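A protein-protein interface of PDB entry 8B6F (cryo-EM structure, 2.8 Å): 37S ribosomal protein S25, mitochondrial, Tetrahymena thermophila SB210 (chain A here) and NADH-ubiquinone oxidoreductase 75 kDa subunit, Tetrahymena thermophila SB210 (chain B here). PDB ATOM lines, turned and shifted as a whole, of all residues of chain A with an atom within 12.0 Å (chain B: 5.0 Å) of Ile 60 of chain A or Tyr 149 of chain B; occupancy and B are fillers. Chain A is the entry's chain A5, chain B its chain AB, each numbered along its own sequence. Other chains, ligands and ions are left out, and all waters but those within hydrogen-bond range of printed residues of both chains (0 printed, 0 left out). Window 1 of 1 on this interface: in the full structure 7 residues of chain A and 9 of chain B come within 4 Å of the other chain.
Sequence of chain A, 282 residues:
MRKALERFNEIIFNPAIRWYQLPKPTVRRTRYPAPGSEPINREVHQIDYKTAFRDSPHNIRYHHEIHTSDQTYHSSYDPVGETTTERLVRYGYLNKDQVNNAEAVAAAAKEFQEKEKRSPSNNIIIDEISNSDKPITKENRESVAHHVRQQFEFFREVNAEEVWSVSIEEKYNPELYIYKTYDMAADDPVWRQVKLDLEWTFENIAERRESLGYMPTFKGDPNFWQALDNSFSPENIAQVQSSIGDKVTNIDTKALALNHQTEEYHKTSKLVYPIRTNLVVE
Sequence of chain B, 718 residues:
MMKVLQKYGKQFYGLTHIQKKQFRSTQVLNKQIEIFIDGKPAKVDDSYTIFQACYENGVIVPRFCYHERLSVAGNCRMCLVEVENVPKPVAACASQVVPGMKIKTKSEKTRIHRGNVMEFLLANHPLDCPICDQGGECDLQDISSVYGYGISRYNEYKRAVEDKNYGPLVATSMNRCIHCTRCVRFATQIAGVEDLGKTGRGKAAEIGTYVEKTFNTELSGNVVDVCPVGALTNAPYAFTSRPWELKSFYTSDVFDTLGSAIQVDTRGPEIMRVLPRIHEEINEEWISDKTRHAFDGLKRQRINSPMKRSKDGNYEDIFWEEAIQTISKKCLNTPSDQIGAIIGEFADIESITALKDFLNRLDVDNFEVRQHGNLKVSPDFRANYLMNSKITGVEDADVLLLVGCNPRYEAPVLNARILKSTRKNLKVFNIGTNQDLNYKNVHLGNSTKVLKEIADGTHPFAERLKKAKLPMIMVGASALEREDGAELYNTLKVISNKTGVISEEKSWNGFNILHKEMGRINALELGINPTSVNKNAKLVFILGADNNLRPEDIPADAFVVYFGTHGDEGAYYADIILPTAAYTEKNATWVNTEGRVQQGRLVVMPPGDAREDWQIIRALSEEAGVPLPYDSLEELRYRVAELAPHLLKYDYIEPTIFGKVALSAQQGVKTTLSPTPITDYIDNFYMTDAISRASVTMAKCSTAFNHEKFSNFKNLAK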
ATOM      1  N   ALA A  52     -14.550 -35.312 -15.587  1.00  0.00           N
ATOM      2  CA  ALA A  52     -15.576 -34.631 -14.812  1.00  0.00           C
ATOM      3  C   ALA A  52     -15.073 -33.273 -14.341  1.00  0.00           C
ATOM      4  O   ALA A  52     -13.875 -33.064 -14.138  1.00  0.00           O
ATOM      5  CB  ALA A  52     -15.988 -35.484 -13.613  1.00  0.00           C
ATOM      6  N   PHE A  53     -16.009 -32.339 -14.166  1.00  0.00           N
ATOM      7  CA  PHE A  53     -15.635 -30.996 -13.738  1.00  0.00           C
ATOM      8  C   PHE A  53     -14.942 -31.028 -12.384  1.00  0.00           C
ATOM      9  O   PHE A  53     -13.938 -30.336 -12.177  1.00  0.00           O
ATOM     10  CB  PHE A  53     -16.874 -30.103 -13.687  1.00  0.00           C
ATOM     11  CG  PHE A  53     -16.621 -28.748 -13.093  1.00  0.00           C
ATOM     12  CD1 PHE A  53     -16.029 -27.748 -13.844  1.00  0.00           C
ATOM     13  CD2 PHE A  53     -16.988 -28.471 -11.788  1.00  0.00           C
ATOM     14  CE1 PHE A  53     -15.799 -26.500 -13.300  1.00  0.00           C
ATOM     15  CE2 PHE A  53     -16.762 -27.227 -11.239  1.00  0.00           C
ATOM     16  CZ  PHE A  53     -16.167 -26.239 -11.995  1.00  0.00           C
ATOM     17  N   ARG A  54     -15.453 -31.832 -11.453  1.00  0.00           N
ATOM     18  CA  ARG A  54     -14.837 -31.937 -10.135  1.00  0.00           C
ATOM     19  C   ARG A  54     -13.400 -32.436 -10.207  1.00  0.00           C
ATOM     20  O   ARG A  54     -12.632 -32.211  -9.266  1.00  0.00           O
ATOM     21  CB  ARG A  54     -15.666 -32.863  -9.243  1.00  0.00           C
ATOM     22  CG  ARG A  54     -15.841 -34.261  -9.812  1.00  0.00           C
ATOM     23  CD  ARG A  54     -16.746 -35.117  -8.946  1.00  0.00           C
ATOM     24  NE  ARG A  54     -16.197 -35.333  -7.614  1.00  0.00           N
ATOM     25  CZ  ARG A  54     -16.632 -36.256  -6.768  1.00  0.00           C
ATOM     26  NH1 ARG A  54     -17.607 -37.089  -7.094  1.00  0.00           N
ATOM     27  NH2 ARG A  54     -16.071 -36.351  -5.566  1.00  0.00           N
ATOM     28  N   ASP A  55     -13.019 -33.110 -11.295  1.00  0.00           N
ATOM     29  CA  ASP A  55     -11.664 -33.611 -11.475  1.00  0.00           C
ATOM     30  C   ASP A  55     -10.881 -32.873 -12.550  1.00  0.00           C
ATOM     31  O   ASP A  55      -9.680 -33.123 -12.696  1.00  0.00           O
ATOM     32  CB  ASP A  55     -11.696 -35.104 -11.828  1.00  0.00           C
ATOM     33  CG  ASP A  55     -12.346 -35.944 -10.750  1.00  0.00           C
ATOM     34  OD1 ASP A  55     -12.636 -35.399  -9.667  1.00  0.00           O
ATOM     35  OD2 ASP A  55     -12.569 -37.149 -10.988  1.00  0.00           O
ATOM     36  N   SER A  56     -11.517 -31.984 -13.301  1.00  0.00           N
ATOM     37  CA  SER A  56     -10.881 -31.314 -14.424  1.00  0.00           C
ATOM     38  C   SER A  56      -9.985 -30.183 -13.947  1.00  0.00           C
ATOM     39  O   SER A  56     -10.062 -29.747 -12.797  1.00  0.00           O
ATOM     40  CB  SER A  56     -11.944 -30.741 -15.348  1.00  0.00           C
ATOM     41  OG  SER A  56     -12.615 -29.696 -14.668  1.00  0.00           O
ATOM     42  N   PRO A  57      -9.107 -29.676 -14.819  1.00  0.00           N
ATOM     43  CA  PRO A  57      -8.299 -28.503 -14.456  1.00  0.00           C
ATOM     44  C   PRO A  57      -9.104 -27.220 -14.318  1.00  0.00           C
ATOM     45  O   PRO A  57      -8.521 -26.179 -13.995  1.00  0.00           O
ATOM     46  CB  PRO A  57      -7.298 -28.388 -15.620  1.00  0.00           C
ATOM     47  CG  PRO A  57      -7.393 -29.669 -16.374  1.00  0.00           C
ATOM     48  CD  PRO A  57      -8.773 -30.179 -16.161  1.00  0.00           C
ATOM     49  N   HIS A  58     -10.415 -27.253 -14.558  1.00  0.00           N
ATOM     50  CA  HIS A  58     -11.262 -26.069 -14.501  1.00  0.00           C
ATOM     51  C   HIS A  58     -11.970 -25.915 -13.163  1.00  0.00           C
ATOM     52  O   HIS A  58     -12.885 -25.094 -13.051  1.00  0.00           O
ATOM     53  CB  HIS A  58     -12.299 -26.110 -15.625  1.00  0.00           C
ATOM     54  CG  HIS A  58     -11.710 -26.309 -16.984  1.00  0.00           C
ATOM     55  ND1 HIS A  58     -11.178 -25.274 -17.724  1.00  0.00           N
ATOM     56  CD2 HIS A  58     -11.573 -27.422 -17.742  1.00  0.00           C
ATOM     57  CE1 HIS A  58     -10.735 -25.743 -18.877  1.00  0.00           C
ATOM     58  NE2 HIS A  58     -10.963 -27.044 -18.913  1.00  0.00           N
ATOM     59  N   ASN A  59     -11.583 -26.687 -12.155  1.00  0.00           N
ATOM     60  CA  ASN A  59     -12.181 -26.623 -10.824  1.00  0.00           C
ATOM     61  C   ASN A  59     -11.130 -26.066  -9.867  1.00  0.00           C
ATOM     62  O   ASN A  59     -10.366 -26.815  -9.258  1.00  0.00           O
ATOM     63  CB  ASN A  59     -12.674 -27.995 -10.385  1.00  0.00           C
ATOM     64  CG  ASN A  59     -13.338 -27.966  -9.028  1.00  0.00           C
ATOM     65  OD1 ASN A  59     -13.894 -26.947  -8.619  1.00  0.00           O
ATOM     66  ND2 ASN A  59     -13.282 -29.085  -8.318  1.00  0.00           N
ATOM     67  N   ILE A  60     -11.098 -24.738  -9.739  1.00  0.00           N
ATOM     68  CA  ILE A  60     -10.137 -24.098  -8.847  1.00  0.00           C
ATOM     69  C   ILE A  60     -10.714 -23.828  -7.463  1.00  0.00           C
ATOM     70  O   ILE A  60      -9.945 -23.686  -6.501  1.00  0.00           O
ATOM     71  CB  ILE A  60      -9.587 -22.796  -9.465  1.00  0.00           C
ATOM     72  CG1 ILE A  60     -10.686 -21.786  -9.833  1.00  0.00           C
ATOM     73  CG2 ILE A  60      -8.754 -23.111 -10.693  1.00  0.00           C
ATOM     74  CD1 ILE A  60     -11.266 -20.994  -8.683  1.00  0.00           C
ATOM     75  N   ARG A  61     -12.033 -23.749  -7.331  1.00  0.00           N
ATOM     76  CA  ARG A  61     -12.634 -23.630  -6.012  1.00  0.00           C
ATOM     77  C   ARG A  61     -12.325 -24.876  -5.196  1.00  0.00           C
ATOM     78  O   ARG A  61     -12.257 -25.987  -5.730  1.00  0.00           O
ATOM     79  CB  ARG A  61     -14.144 -23.428  -6.130  1.00  0.00           C
ATOM     80  CG  ARG A  61     -14.832 -23.156  -4.804  1.00  0.00           C
ATOM     81  CD  ARG A  61     -16.337 -23.029  -4.969  1.00  0.00           C
ATOM     82  NE  ARG A  61     -16.707 -21.897  -5.810  1.00  0.00           N
ATOM     83  CZ  ARG A  61     -17.955 -21.547  -6.089  1.00  0.00           C
ATOM     84  NH1 ARG A  61     -18.987 -22.219  -5.606  1.00  0.00           N
ATOM     85  NH2 ARG A  61     -18.174 -20.496  -6.873  1.00  0.00           N
ATOM     86  N   TYR A  62     -12.129 -24.687  -3.895  1.00  0.00           N
ATOM     87  CA  TYR A  62     -11.724 -25.732  -2.962  1.00  0.00           C
ATOM     88  C   TYR A  62     -10.285 -26.176  -3.180  1.00  0.00           C
ATOM     89  O   TYR A  62      -9.867 -27.193  -2.616  1.00  0.00           O
ATOM     90  CB  TYR A  62     -12.646 -26.955  -3.039  1.00  0.00           C
ATOM     91  CG  TYR A  62     -14.106 -26.618  -2.853  1.00  0.00           C
ATOM     92  CD1 TYR A  62     -14.597 -26.235  -1.613  1.00  0.00           C
ATOM     93  CD2 TYR A  62     -14.995 -26.689  -3.917  1.00  0.00           C
ATOM     94  CE1 TYR A  62     -15.932 -25.926  -1.439  1.00  0.00           C
ATOM     95  CE2 TYR A  62     -16.330 -26.384  -3.753  1.00  0.00           C
ATOM     96  CZ  TYR A  62     -16.792 -26.002  -2.512  1.00  0.00           C
ATOM     97  OH  TYR A  62     -18.122 -25.698  -2.343  1.00  0.00           O
ATOM     98  N   HIS A  63      -9.514 -25.448  -3.989  1.00  0.00           N
ATOM     99  CA  HIS A  63      -8.088 -25.732  -4.093  1.00  0.00           C
ATOM    100  C   HIS A  63      -7.406 -25.552  -2.743  1.00  0.00           C
ATOM    101  O   HIS A  63      -6.572 -26.372  -2.345  1.00  0.00           O
ATOM    102  CB  HIS A  63      -7.450 -24.823  -5.144  1.00  0.00           C
ATOM    103  CG  HIS A  63      -5.966 -24.972  -5.254  1.00  0.00           C
ATOM    104  ND1 HIS A  63      -5.366 -26.104  -5.761  1.00  0.00           N
ATOM    105  CD2 HIS A  63      -4.959 -24.128  -4.925  1.00  0.00           C
ATOM    106  CE1 HIS A  63      -4.054 -25.952  -5.738  1.00  0.00           C
ATOM    107  NE2 HIS A  63      -3.780 -24.762  -5.235  1.00  0.00           N
ATOM    108  N   HIS A  64      -7.750 -24.485  -2.027  1.00  0.00           N
ATOM    109  CA  HIS A  64      -7.281 -24.299  -0.663  1.00  0.00           C
ATOM    110  C   HIS A  64      -8.069 -25.193   0.283  1.00  0.00           C
ATOM    111  O   HIS A  64      -9.273 -25.398   0.110  1.00  0.00           O
ATOM    112  CB  HIS A  64      -7.420 -22.837  -0.241  1.00  0.00           C
ATOM    113  CG  HIS A  64      -6.512 -21.908  -0.984  1.00  0.00           C
ATOM    114  ND1 HIS A  64      -5.279 -21.527  -0.499  1.00  0.00           N
ATOM    115  CD2 HIS A  64      -6.654 -21.285  -2.177  1.00  0.00           C
ATOM    116  CE1 HIS A  64      -4.703 -20.710  -1.361  1.00  0.00           C
ATOM    117  NE2 HIS A  64      -5.516 -20.545  -2.387  1.00  0.00           N
ATOM    118  N   GLU A  65      -7.385 -25.719   1.294  1.00  0.00           N
ATOM    119  CA  GLU A  65      -7.995 -26.656   2.229  1.00  0.00           C
ATOM    120  C   GLU A  65      -8.849 -25.881   3.224  1.00  0.00           C
ATOM    121  O   GLU A  65      -8.321 -25.186   4.098  1.00  0.00           O
ATOM    122  CB  GLU A  65      -6.920 -27.472   2.939  1.00  0.00           C
ATOM    123  CG  GLU A  65      -5.946 -28.147   1.987  1.00  0.00           C
ATOM    124  CD  GLU A  65      -4.897 -28.964   2.709  1.00  0.00           C
ATOM    125  OE1 GLU A  65      -5.096 -29.258   3.906  1.00  0.00           O
ATOM    126  OE2 GLU A  65      -3.873 -29.308   2.082  1.00  0.00           O
ATOM    127  N   ILE A  66     -10.172 -25.998   3.096  1.00  0.00           N
ATOM    128  CA  ILE A  66     -11.067 -25.302   4.015  1.00  0.00           C
ATOM    129  C   ILE A  66     -10.973 -25.906   5.412  1.00  0.00           C
ATOM    130  O   ILE A  66     -11.034 -25.188   6.417  1.00  0.00           O
ATOM    131  CB  ILE A  66     -12.512 -25.322   3.484  1.00  0.00           C
ATOM    132  CG1 ILE A  66     -13.041 -26.759   3.414  1.00  0.00           C
ATOM    133  CG2 ILE A  66     -12.569 -24.647   2.117  1.00  0.00           C
ATOM    134  CD1 ILE A  66     -14.449 -26.882   2.869  1.00  0.00           C
ATOM    135  N   ARG B 111     -15.626 -16.176   1.845  1.00  0.00           N
ATOM    136  CA  ARG B 111     -14.458 -16.691   1.139  1.00  0.00           C
ATOM    137  C   ARG B 111     -14.741 -16.836  -0.349  1.00  0.00           C
ATOM    138  O   ARG B 111     -13.912 -16.462  -1.186  1.00  0.00           O
ATOM    139  CB  ARG B 111     -14.035 -18.034   1.737  1.00  0.00           C
ATOM    140  CG  ARG B 111     -13.012 -18.793   0.902  1.00  0.00           C
ATOM    141  CD  ARG B 111     -12.671 -20.135   1.520  1.00  0.00           C
ATOM    142  NE  ARG B 111     -11.908 -20.968   0.600  1.00  0.00           N
ATOM    143  CZ  ARG B 111     -12.440 -21.720  -0.355  1.00  0.00           C
ATOM    144  NH1 ARG B 111     -13.748 -21.776  -0.543  1.00  0.00           N
ATOM    145  NH2 ARG B 111     -11.640 -22.432  -1.142  1.00  0.00           N
ATOM    146  N   ILE B 112     -15.907 -17.382  -0.698  1.00  0.00           N
ATOM    147  CA  ILE B 112     -16.252 -17.567  -2.103  1.00  0.00           C
ATOM    148  C   ILE B 112     -16.393 -16.219  -2.795  1.00  0.00           C
ATOM    149  O   ILE B 112     -15.950 -16.041  -3.936  1.00  0.00           O
ATOM    150  CB  ILE B 112     -17.532 -18.415  -2.229  1.00  0.00           C
ATOM    151  CG1 ILE B 112     -17.291 -19.839  -1.714  1.00  0.00           C
ATOM    152  CG2 ILE B 112     -18.024 -18.448  -3.672  1.00  0.00           C
ATOM    153  CD1 ILE B 112     -16.270 -20.638  -2.504  1.00  0.00           C
ATOM    154  N   GLY B 115     -12.939 -14.886  -3.442  1.00  0.00           N
ATOM    155  CA  GLY B 115     -12.306 -15.643  -4.506  1.00  0.00           C
ATOM    156  C   GLY B 115     -12.845 -15.292  -5.879  1.00  0.00           C
ATOM    157  O   GLY B 115     -12.084 -15.162  -6.840  1.00  0.00           O
ATOM    158  N   ASN B 116     -14.166 -15.144  -5.995  1.00  0.00           N
ATOM    159  CA  ASN B 116     -14.752 -14.784  -7.282  1.00  0.00           C
ATOM    160  C   ASN B 116     -14.264 -13.418  -7.744  1.00  0.00           C
ATOM    161  O   ASN B 116     -13.877 -13.243  -8.903  1.00  0.00           O
ATOM    162  CB  ASN B 116     -16.276 -14.791  -7.184  1.00  0.00           C
ATOM    163  CG  ASN B 116     -16.820 -16.107  -6.680  1.00  0.00           C
ATOM    164  OD1 ASN B 116     -16.159 -17.139  -6.768  1.00  0.00           O
ATOM    165  ND2 ASN B 116     -18.040 -16.080  -6.159  1.00  0.00           N
ATOM    166  N   GLU B 119     -10.629 -13.598  -8.788  1.00  0.00           N
ATOM    167  CA  GLU B 119     -10.476 -14.266 -10.074  1.00  0.00           C
ATOM    168  C   GLU B 119     -10.840 -13.331 -11.219  1.00  0.00           C
ATOM    169  O   GLU B 119     -10.144 -13.286 -12.240  1.00  0.00           O
ATOM    170  CB  GLU B 119     -11.341 -15.524 -10.116  1.00  0.00           C
ATOM    171  CG  GLU B 119     -11.219 -16.314 -11.409  1.00  0.00           C
ATOM    172  CD  GLU B 119     -12.103 -17.544 -11.423  1.00  0.00           C
ATOM    173  OE1 GLU B 119     -12.992 -17.647 -10.553  1.00  0.00           O
ATOM    174  OE2 GLU B 119     -11.908 -18.408 -12.302  1.00  0.00           O
ATOM    175  N   SER B 144      -4.495 -11.529  -3.275  1.00  0.00           N
ATOM    176  CA  SER B 144      -4.620 -12.788  -3.998  1.00  0.00           C
ATOM    177  C   SER B 144      -4.034 -13.942  -3.199  1.00  0.00           C
ATOM    178  O   SER B 144      -4.545 -15.064  -3.266  1.00  0.00           O
ATOM    179  CB  SER B 144      -3.931 -12.683  -5.358  1.00  0.00           C
ATOM    180  OG  SER B 144      -3.985 -13.917  -6.051  1.00  0.00           O
ATOM    181  N   TYR B 147      -6.603 -14.095   0.365  1.00  0.00           N
ATOM    182  CA  TYR B 147      -8.048 -14.265   0.270  1.00  0.00           C
ATOM    183  C   TYR B 147      -8.497 -15.000  -0.983  1.00  0.00           C
ATOM    184  O   TYR B 147      -9.406 -15.829  -0.908  1.00  0.00           O
ATOM    185  CB  TYR B 147      -8.740 -12.895   0.322  1.00  0.00           C
ATOM    186  CG  TYR B 147      -8.441 -12.112   1.580  1.00  0.00           C
ATOM    187  CD1 TYR B 147      -9.166 -12.328   2.744  1.00  0.00           C
ATOM    188  CD2 TYR B 147      -7.438 -11.154   1.601  1.00  0.00           C
ATOM    189  CE1 TYR B 147      -8.897 -11.616   3.894  1.00  0.00           C
ATOM    190  CE2 TYR B 147      -7.161 -10.435   2.746  1.00  0.00           C
ATOM    191  CZ  TYR B 147      -7.894 -10.670   3.888  1.00  0.00           C
ATOM    192  OH  TYR B 147      -7.622  -9.959   5.033  1.00  0.00           O
ATOM    193  N   GLY B 148      -7.896 -14.716  -2.133  1.00  0.00           N
ATOM    194  CA  GLY B 148      -8.327 -15.335  -3.366  1.00  0.00           C
ATOM    195  C   GLY B 148      -7.855 -16.772  -3.498  1.00  0.00           C
ATOM    196  O   GLY B 148      -7.093 -17.289  -2.683  1.00  0.00           O
ATOM    197  N   TYR B 149      -8.333 -17.423  -4.555  1.00  0.00           N
ATOM    198  CA  TYR B 149      -7.928 -18.790  -4.842  1.00  0.00           C
ATOM    199  C   TYR B 149      -6.460 -18.821  -5.264  1.00  0.00           C
ATOM    200  O   TYR B 149      -5.848 -17.794  -5.574  1.00  0.00           O
ATOM    201  CB  TYR B 149      -8.805 -19.397  -5.936  1.00  0.00           C
ATOM    202  CG  TYR B 149     -10.289 -19.344  -5.657  1.00  0.00           C
ATOM    203  CD1 TYR B 149     -10.836 -20.006  -4.566  1.00  0.00           C
ATOM    204  CD2 TYR B 149     -11.148 -18.649  -6.498  1.00  0.00           C
ATOM    205  CE1 TYR B 149     -12.195 -19.967  -4.314  1.00  0.00           C
ATOM    206  CE2 TYR B 149     -12.507 -18.605  -6.256  1.00  0.00           C
ATOM    207  CZ  TYR B 149     -13.024 -19.265  -5.163  1.00  0.00           C
ATOM    208  OH  TYR B 149     -14.376 -19.225  -4.921  1.00  0.00           O
ATOM    209  N   GLY B 150      -5.891 -20.023  -5.272  1.00  0.00           N
ATOM    210  CA  GLY B 150      -4.480 -20.182  -5.562  1.00  0.00           C
ATOM    211  C   GLY B 150      -4.163 -20.503  -7.007  1.00  0.00           C
ATOM    212  O   GLY B 150      -2.991 -20.519  -7.393  1.00  0.00           O
ATOM    213  N   ILE B 151      -5.187 -20.763  -7.819  1.00  0.00           N
ATOM    214  CA  ILE B 151      -5.000 -21.123  -9.218  1.00  0.00           C
ATOM    215  C   ILE B 151      -6.083 -20.447 -10.045  1.00  0.00           C
ATOM    216  O   ILE B 151      -7.189 -20.186  -9.563  1.00  0.00           O
ATOM    217  CB  ILE B 151      -5.019 -22.656  -9.419  1.00  0.00           C
ATOM    218  CG1 ILE B 151      -3.850 -23.286  -8.657  1.00  0.00           C
ATOM    219  CG2 ILE B 151      -4.961 -23.011 -10.904  1.00  0.00           C
ATOM    220  CD1 ILE B 151      -3.708 -24.785  -8.826  1.00  0.00           C
ATOM    221  N   SER B 152      -5.753 -20.156 -11.300  1.00  0.00           N
ATOM    222  CA  SER B 152      -6.640 -19.452 -12.211  1.00  0.00           C
ATOM    223  C   SER B 152      -7.155 -20.399 -13.287  1.00  0.00           C
ATOM    224  O   SER B 152      -6.481 -21.361 -13.666  1.00  0.00           O
ATOM    225  CB  SER B 152      -5.919 -18.269 -12.866  1.00  0.00           C
ATOM    226  OG  SER B 152      -6.799 -17.522 -13.688  1.00  0.00           O
ATOM    227  N   ARG B 153      -8.363 -20.115 -13.775  1.00  0.00           N
ATOM    228  CA  ARG B 153      -8.977 -20.892 -14.843  1.00  0.00           C
ATOM    229  C   ARG B 153      -8.955 -20.188 -16.190  1.00  0.00           C
ATOM    230  O   ARG B 153      -9.046 -20.859 -17.223  1.00  0.00           O
ATOM    231  CB  ARG B 153     -10.434 -21.221 -14.498  1.00  0.00           C
ATOM    232  CG  ARG B 153     -10.595 -22.103 -13.285  1.00  0.00           C
ATOM    233  CD  ARG B 153     -12.059 -22.369 -12.987  1.00  0.00           C
ATOM    234  NE  ARG B 153     -12.790 -21.148 -12.677  1.00  0.00           N
ATOM    235  CZ  ARG B 153     -14.059 -21.112 -12.297  1.00  0.00           C
ATOM    236  NH1 ARG B 153     -14.772 -22.218 -12.163  1.00  0.00           N
ATOM    237  NH2 ARG B 153     -14.627 -19.937 -12.043  1.00  0.00           N
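Printed residues of chain B that touch a printed residue of chain A: Arg 111, Ile 112, Asn 116, Gly 148, Tyr 149, Gly 150, Ile 151 and Arg 153. Hydrophobic or aromatic side chains of chain A that line the printed part of chain B: Ile 60, His 63, His 64 and Ile 66. Among the printed residues, no Asp or Glu carboxylate lies within 4 Å of a Lys or Arg side-chain nitrogen of the other chain.
The backbone NH (N) of Gly 150 of chain B is in hydrogen-bond range of a ring nitrogen (NE2) of His 64 of chain A.
Ala 52 of chain A touches none of the printed residues of chain B. Pro 57 of chain A touches none of the printed residues of chain B. Ile 60 of chain A touches just these residues of chain B: Tyr 149, Ile 151 and Arg 153. Printed residues of chain B within 4 Å of Tyr 62 of chain A: Arg 111. Printed residues of chain B within 4 Å of His 64 of chain A: Arg 111, Gly 148, Tyr 149 and Gly 150. Of the printed residues of chain B, Ile 66 of chain A touches Arg 111. Of the printed residues of chain A, Arg 111 of chain B touches Tyr 62 (3.6 Å), His 64 (3.996 Å) and Ile 66 (3.8 Å). Ile 112 of chain B touches one residue of chain A. No residue of chain A comes within 4 Å of Gly 115 of chain B. Printed residues of chain A within 4 Å of Asn 116 of chain B: Arg 61. No residue of chain A comes within 4 Å of Glu 119 of chain B. Gly 148 of chain B touches just one residue of chain A: His 64 (3.6 Å). Of the printed residues of chain A, Tyr 149 of chain B touches Ile 60, Arg 61 and His 64. Gly 150 of chain B touches just one residue of chain A: His 64 (3.0 Å). Of chain A, only Ile 60 (3.5 Å) and His 63 (3.3 Å) come within 4 Å of Ile 151 of chain B. No residue of chain A comes within 4 Å of Ser 152 of chain B. Of chain A, only His 58 and Ile 60 come within 4 Å of Arg 153 of chain B. The nearest residue of chain A that does not touch Tyr 149 of chain B is Tyr 62 of chain A (4.7 Å).
OD1 of Asn 116 of chain B is in hydrogen-bond range of OH of Tyr 149 of chain B (3.3 Å). The side-chain amide oxygen of Asn 59 of chain A sits close to the backbone carbonyl oxygen of Arg 61 of chain A, at 3.5 Å. The side-chain carboxylate (OE2) of Glu 119 of chain B lies within salt-bridge range of the guanidinium group (NE) of Arg 153 of chain B (2.9 Å). The side-chain hydroxyl (OG) of Ser 56 of chain A lies close to the backbone NH (N) of His 58 of chain A, at 3.3 Å. The backbone carbonyl oxygen of Ile 112 of chain B lies close to the side-chain amide oxygen of Asn 116 of chain B, at 3.0 Å.
Arg 153 of chain B touches His 58 of chain A. Ile 60 of chain A touches Tyr 149 of chain B (CD1 to CD2, 3.2 Å). CG2 of Ile 60 of chain A touches O of Ile 151 of chain B, at 3.5 Å. NE of Arg 61 of chain A touches OH of Tyr 149 of chain B, at 3.7 Å. Tyr 62 of chain A touches Arg 111 of chain B (N to NH2, 3.6 Å). His 63 of chain A touches Ile 151 of chain B (CE1 to CD1, 3.3 Å). O of His 64 of chain A touches NH2 of Arg 111 of chain B (3.996 Å). NE2 of His 64 of chain A touches O of Gly 148 of chain B, 3.6 Å away. His 64 of chain A touches Tyr 149 of chain B. Ile 66 of chain A touches Arg 111 of chain B.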
